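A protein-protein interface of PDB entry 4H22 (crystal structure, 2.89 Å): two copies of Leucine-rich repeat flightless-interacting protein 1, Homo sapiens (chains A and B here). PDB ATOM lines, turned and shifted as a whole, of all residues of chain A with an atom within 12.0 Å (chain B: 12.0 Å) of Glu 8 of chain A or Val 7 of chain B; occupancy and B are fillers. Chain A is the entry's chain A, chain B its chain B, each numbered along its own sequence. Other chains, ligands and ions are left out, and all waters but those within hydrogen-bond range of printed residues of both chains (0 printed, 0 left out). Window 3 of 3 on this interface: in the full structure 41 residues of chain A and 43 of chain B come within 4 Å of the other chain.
No residue of chain B comes within 4 Å of Glu 9 of chain A.
Lys 10 of chain A touches just one residue of chain B: Tyr 11 (3.9 Å).
Printed residues of chain B within 4 Å of Ala 14 of chain A: Met 15.
Of the printed residues of chain A, Val 7 of chain B touches Glu 8.
No residue of chain A comes within 4 Å of Glu 9 of chain B.
Of chain A, only Tyr 11 comes within 4 Å of Lys 10 of chain B.
Tyr 11 of chain B touches just these residues of chain A: Lys 10 (3.9 Å) and Tyr 11 (3.6 Å).
Lys 13 of chain B touches none of the printed residues of chain A.
Printed residues of chain A within 4 Å of Met 15 of chain B: Ala 14.
The nearest residue of chain B that does not touch Glu 8 of chain A is Tyr 11 of chain B (5.3 Å).
The nearest residue of chain A that does not touch Val 7 of chain B is Tyr 11 of chain A (5.3 Å).
Lys 10 of chain A touches Tyr 11 of chain B, and with the chains exchanged Tyr 11 of chain A touches Lys 10 of chain B.
Tyr 11 of chain A touches its own counterpart, Tyr 11 of chain B.
Ala 14 of chain A touches Met 15 of chain B, but with the chains exchanged Met 15 of chain A does not touch Ala 14 of chain B (5.3 Å).
Positions printed for both chains: 8, 9, 10, 11, 12, 13, 14, 15 and 16.
Of the 5 pairs that touch across the chains among the printed residues, 3 have their exchanged pair printed and touching as well.
CB of Glu 8 of chain A touches N of Val 7 of chain B (3.6 Å).
C of Lys 10 of chain A touches CE1 of Tyr 11 of chain B (3.9 Å).
Tyr 11 of chain A touches Lys 10 of chain B.
Tyr 11 of chain B touches Tyr 11 of chain A (CD1 to CA, 3.6 Å).
Ala 14 of chain A touches Met 15 of chain B (CB to SD, 3.9 Å).
Printed residues of chain A that touch a printed residue of chain B: Glu 8, Lys 10, Tyr 11 and Ala 14.
Of the 10 printed residues of chain B, 4 touch a printed residue of chain A.
Hydrophobic or aromatic side chains of chain B that line the printed part of chain A: Tyr 11 and Met 15.
Among the printed residues, no Asp or Glu carboxylate lies within 4 Å of a Lys or Arg side-chain nitrogen of the other chain.
The side-chain hydroxyl (OH) of Tyr 11 of chain A sits at hydrogen-bond distance from the side-chain sulfur (SD) of Met 15 of chain A, at 3.4 Å.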
ATOM      1  N   GLU A   8      17.152  17.116  -3.662  1.00  0.00           N
ATOM      2  CA  GLU A   8      18.319  17.627  -2.884  1.00  0.00           C
ATOM      3  C   GLU A   8      18.999  18.818  -3.574  1.00  0.00           C
ATOM      4  O   GLU A   8      20.132  19.178  -3.242  1.00  0.00           O
ATOM      5  CB  GLU A   8      19.322  16.495  -2.630  1.00  0.00           C
ATOM      6  N   GLU A   9      18.292  19.432  -4.524  1.00  0.00           N
ATOM      7  CA  GLU A   9      18.819  20.561  -5.303  1.00  0.00           C
ATOM      8  C   GLU A   9      18.176  21.887  -4.900  1.00  0.00           C
ATOM      9  O   GLU A   9      18.840  22.937  -4.879  1.00  0.00           O
ATOM     10  CB  GLU A   9      18.610  20.325  -6.802  1.00  0.00           C
ATOM     11  CG  GLU A   9      19.325  19.093  -7.360  1.00  0.00           C
ATOM     12  CD  GLU A   9      19.373  19.095  -8.885  1.00  0.00           C
ATOM     13  OE1 GLU A   9      18.467  19.693  -9.519  1.00  0.00           O
ATOM     14  OE2 GLU A   9      20.321  18.498  -9.449  1.00  0.00           O
ATOM     15  N   LYS A  10      16.874  21.830  -4.604  1.00  0.00           N
ATOM     16  CA  LYS A  10      16.132  22.985  -4.102  1.00  0.00           C
ATOM     17  C   LYS A  10      16.386  23.173  -2.608  1.00  0.00           C
ATOM     18  O   LYS A  10      16.054  24.215  -2.039  1.00  0.00           O
ATOM     19  CB  LYS A  10      14.628  22.813  -4.363  1.00  0.00           C
ATOM     20  N   TYR A  11      16.978  22.151  -1.988  1.00  0.00           N
ATOM     21  CA  TYR A  11      17.378  22.186  -0.581  1.00  0.00           C
ATOM     22  C   TYR A  11      18.302  23.357  -0.279  1.00  0.00           C
ATOM     23  O   TYR A  11      18.309  23.879   0.838  1.00  0.00           O
ATOM     24  CB  TYR A  11      18.058  20.873  -0.196  1.00  0.00           C
ATOM     25  CG  TYR A  11      18.711  20.895   1.162  1.00  0.00           C
ATOM     26  CD1 TYR A  11      17.964  20.686   2.317  1.00  0.00           C
ATOM     27  CD2 TYR A  11      20.080  21.129   1.293  1.00  0.00           C
ATOM     28  CE1 TYR A  11      18.558  20.707   3.567  1.00  0.00           C
ATOM     29  CE2 TYR A  11      20.686  21.150   2.536  1.00  0.00           C
ATOM     30  CZ  TYR A  11      19.919  20.938   3.669  1.00  0.00           C
ATOM     31  OH  TYR A  11      20.512  20.960   4.905  1.00  0.00           O
ATOM     32  N   LYS A  12      19.095  23.745  -1.274  1.00  0.00           N
ATOM     33  CA  LYS A  12      19.886  24.961  -1.204  1.00  0.00           C
ATOM     34  C   LYS A  12      18.956  26.155  -0.976  1.00  0.00           C
ATOM     35  O   LYS A  12      19.147  26.936  -0.042  1.00  0.00           O
ATOM     36  CB  LYS A  12      20.679  25.147  -2.503  1.00  0.00           C
ATOM     37  CG  LYS A  12      21.950  25.972  -2.356  1.00  0.00           C
ATOM     38  CD  LYS A  12      22.177  26.894  -3.544  1.00  0.00           C
ATOM     39  CE  LYS A  12      21.355  28.171  -3.418  1.00  0.00           C
ATOM     40  NZ  LYS A  12      21.628  29.129  -4.522  1.00  0.00           N
ATOM     41  N   LYS A  13      17.926  26.261  -1.810  1.00  0.00           N
ATOM     42  CA  LYS A  13      17.051  27.428  -1.816  1.00  0.00           C
ATOM     43  C   LYS A  13      16.066  27.441  -0.644  1.00  0.00           C
ATOM     44  O   LYS A  13      15.559  28.500  -0.264  1.00  0.00           O
ATOM     45  CB  LYS A  13      16.307  27.521  -3.150  1.00  0.00           C
ATOM     46  CG  LYS A  13      16.345  28.906  -3.774  1.00  0.00           C
ATOM     47  CD  LYS A  13      15.329  29.037  -4.900  1.00  0.00           C
ATOM     48  CE  LYS A  13      15.366  30.430  -5.510  1.00  0.00           C
ATOM     49  NZ  LYS A  13      14.064  30.795  -6.154  1.00  0.00           N
ATOM     50  N   ALA A  14      15.796  26.265  -0.080  1.00  0.00           N
ATOM     51  CA  ALA A  14      14.951  26.162   1.105  1.00  0.00           C
ATOM     52  C   ALA A  14      15.686  26.756   2.290  1.00  0.00           C
ATOM     53  O   ALA A  14      15.085  27.423   3.133  1.00  0.00           O
ATOM     54  CB  ALA A  14      14.572  24.717   1.383  1.00  0.00           C
ATOM     55  N   MET A  15      16.993  26.522   2.335  1.00  0.00           N
ATOM     56  CA  MET A  15      17.839  27.086   3.375  1.00  0.00           C
ATOM     57  C   MET A  15      18.018  28.594   3.245  1.00  0.00           C
ATOM     58  O   MET A  15      18.107  29.294   4.255  1.00  0.00           O
ATOM     59  CB  MET A  15      19.194  26.389   3.406  1.00  0.00           C
ATOM     60  CG  MET A  15      19.208  25.116   4.238  1.00  0.00           C
ATOM     61  SD  MET A  15      20.835  24.326   4.295  1.00  0.00           S
ATOM     62  CE  MET A  15      21.784  25.511   5.241  1.00  0.00           C
ATOM     63  N   VAL A  16      18.065  29.092   2.011  1.00  0.00           N
ATOM     64  CA  VAL A  16      18.189  30.531   1.763  1.00  0.00           C
ATOM     65  C   VAL A  16      16.902  31.233   2.183  1.00  0.00           C
ATOM     66  O   VAL A  16      16.928  32.257   2.871  1.00  0.00           O
ATOM     67  CB  VAL A  16      18.510  30.835   0.280  1.00  0.00           C
ATOM     68  CG1 VAL A  16      18.243  32.296  -0.057  1.00  0.00           C
ATOM     69  CG2 VAL A  16      19.955  30.481  -0.038  1.00  0.00           C
ATOM     70  N   VAL B   7      19.107  15.063   0.665  1.00  0.00           N
ATOM     71  CA  VAL B   7      18.604  14.044   1.631  1.00  0.00           C
ATOM     72  C   VAL B   7      17.161  14.352   2.009  1.00  0.00           C
ATOM     73  O   VAL B   7      16.826  15.486   2.349  1.00  0.00           O
ATOM     74  CB  VAL B   7      19.504  13.943   2.887  1.00  0.00           C
ATOM     75  CG1 VAL B   7      18.793  13.234   4.033  1.00  0.00           C
ATOM     76  CG2 VAL B   7      20.801  13.221   2.549  1.00  0.00           C
ATOM     77  N   GLU B   8      16.314  13.331   1.929  1.00  0.00           N
ATOM     78  CA  GLU B   8      14.906  13.443   2.289  1.00  0.00           C
ATOM     79  C   GLU B   8      14.706  14.106   3.653  1.00  0.00           C
ATOM     80  O   GLU B   8      13.981  15.094   3.756  1.00  0.00           O
ATOM     81  CB  GLU B   8      14.236  12.065   2.262  1.00  0.00           C
ATOM     82  N   GLU B   9      15.374  13.578   4.680  1.00  0.00           N
ATOM     83  CA  GLU B   9      15.169  14.025   6.063  1.00  0.00           C
ATOM     84  C   GLU B   9      15.671  15.437   6.372  1.00  0.00           C
ATOM     85  O   GLU B   9      15.060  16.148   7.173  1.00  0.00           O
ATOM     86  CB  GLU B   9      15.746  13.017   7.065  1.00  0.00           C
ATOM     87  CG  GLU B   9      14.723  12.026   7.615  1.00  0.00           C
ATOM     88  CD  GLU B   9      13.622  12.685   8.443  1.00  0.00           C
ATOM     89  OE1 GLU B   9      13.930  13.555   9.288  1.00  0.00           O
ATOM     90  OE2 GLU B   9      12.440  12.324   8.258  1.00  0.00           O
ATOM     91  N   LYS B  10      16.771  15.843   5.740  1.00  0.00           N
ATOM     92  CA  LYS B  10      17.291  17.204   5.903  1.00  0.00           C
ATOM     93  C   LYS B  10      16.366  18.235   5.240  1.00  0.00           C
ATOM     94  O   LYS B  10      16.011  19.244   5.856  1.00  0.00           O
ATOM     95  CB  LYS B  10      18.724  17.316   5.368  1.00  0.00           C
ATOM     96  N   TYR B  11      15.968  17.961   3.997  1.00  0.00           N
ATOM     97  CA  TYR B  11      15.025  18.803   3.255  1.00  0.00           C
ATOM     98  C   TYR B  11      13.652  18.855   3.919  1.00  0.00           C
ATOM     99  O   TYR B  11      12.994  19.895   3.900  1.00  0.00           O
ATOM    100  CB  TYR B  11      14.886  18.301   1.816  1.00  0.00           C
ATOM    101  CG  TYR B  11      14.019  19.163   0.918  1.00  0.00           C
ATOM    102  CD1 TYR B  11      14.596  20.023  -0.014  1.00  0.00           C
ATOM    103  CD2 TYR B  11      12.626  19.096   0.976  1.00  0.00           C
ATOM    104  CE1 TYR B  11      13.814  20.805  -0.852  1.00  0.00           C
ATOM    105  CE2 TYR B  11      11.836  19.876   0.146  1.00  0.00           C
ATOM    106  CZ  TYR B  11      12.435  20.727  -0.766  1.00  0.00           C
ATOM    107  OH  TYR B  11      11.659  21.502  -1.595  1.00  0.00           O
ATOM    108  N   LYS B  12      13.216  17.727   4.481  1.00  0.00           N
ATOM    109  CA  LYS B  12      11.946  17.671   5.192  1.00  0.00           C
ATOM    110  C   LYS B  12      11.948  18.703   6.302  1.00  0.00           C
ATOM    111  O   LYS B  12      11.177  19.659   6.258  1.00  0.00           O
ATOM    112  CB  LYS B  12      11.668  16.276   5.763  1.00  0.00           C
ATOM    113  CG  LYS B  12      10.382  16.202   6.577  1.00  0.00           C
ATOM    114  CD  LYS B  12      10.089  14.800   7.082  1.00  0.00           C
ATOM    115  CE  LYS B  12       8.706  14.738   7.712  1.00  0.00           C
ATOM    116  NZ  LYS B  12       8.307  13.342   8.038  1.00  0.00           N
ATOM    117  N   LYS B  13      12.841  18.521   7.272  1.00  0.00           N
ATOM    118  CA  LYS B  13      12.949  19.430   8.410  1.00  0.00           C
ATOM    119  C   LYS B  13      13.023  20.886   7.964  1.00  0.00           C
ATOM    120  O   LYS B  13      12.510  21.766   8.649  1.00  0.00           O
ATOM    121  CB  LYS B  13      14.159  19.080   9.283  1.00  0.00           C
ATOM    122  CG  LYS B  13      14.056  17.750  10.016  1.00  0.00           C
ATOM    123  CD  LYS B  13      14.888  17.748  11.292  1.00  0.00           C
ATOM    124  CE  LYS B  13      15.453  16.368  11.607  1.00  0.00           C
ATOM    125  NZ  LYS B  13      14.416  15.303  11.723  1.00  0.00           N
ATOM    126  N   ALA B  14      13.635  21.119   6.802  1.00  0.00           N
ATOM    127  CA  ALA B  14      13.822  22.461   6.253  1.00  0.00           C
ATOM    128  C   ALA B  14      12.510  23.141   5.876  1.00  0.00           C
ATOM    129  O   ALA B  14      12.235  24.246   6.336  1.00  0.00           O
ATOM    130  CB  ALA B  14      14.766  22.424   5.061  1.00  0.00           C
ATOM    131  N   MET B  15      11.706  22.487   5.041  1.00  0.00           N
ATOM    132  CA  MET B  15      10.396  23.024   4.665  1.00  0.00           C
ATOM    133  C   MET B  15       9.401  22.954   5.824  1.00  0.00           C
ATOM    134  O   MET B  15       8.407  23.674   5.838  1.00  0.00           O
ATOM    135  CB  MET B  15       9.834  22.315   3.429  1.00  0.00           C
ATOM    136  CG  MET B  15      10.628  22.543   2.149  1.00  0.00           C
ATOM    137  SD  MET B  15      10.669  24.248   1.554  1.00  0.00           S
ATOM    138  CE  MET B  15       9.082  24.402   0.724  1.00  0.00           C
ATOM    139  N   VAL B  16       9.678  22.084   6.789  1.00  0.00           N
ATOM    140  CA  VAL B  16       8.921  22.052   8.038  1.00  0.00           C
ATOM    141  C   VAL B  16       9.293  23.268   8.888  1.00  0.00           C
ATOM    142  O   VAL B  16       8.439  23.872   9.538  1.00  0.00           O
ATOM    143  CB  VAL B  16       9.157  20.736   8.814  1.00  0.00           C
ATOM    144  CG1 VAL B  16       8.599  20.811  10.230  1.00  0.00           C
ATOM    145  CG2 VAL B  16       8.524  19.573   8.067  1.00  0.00           C
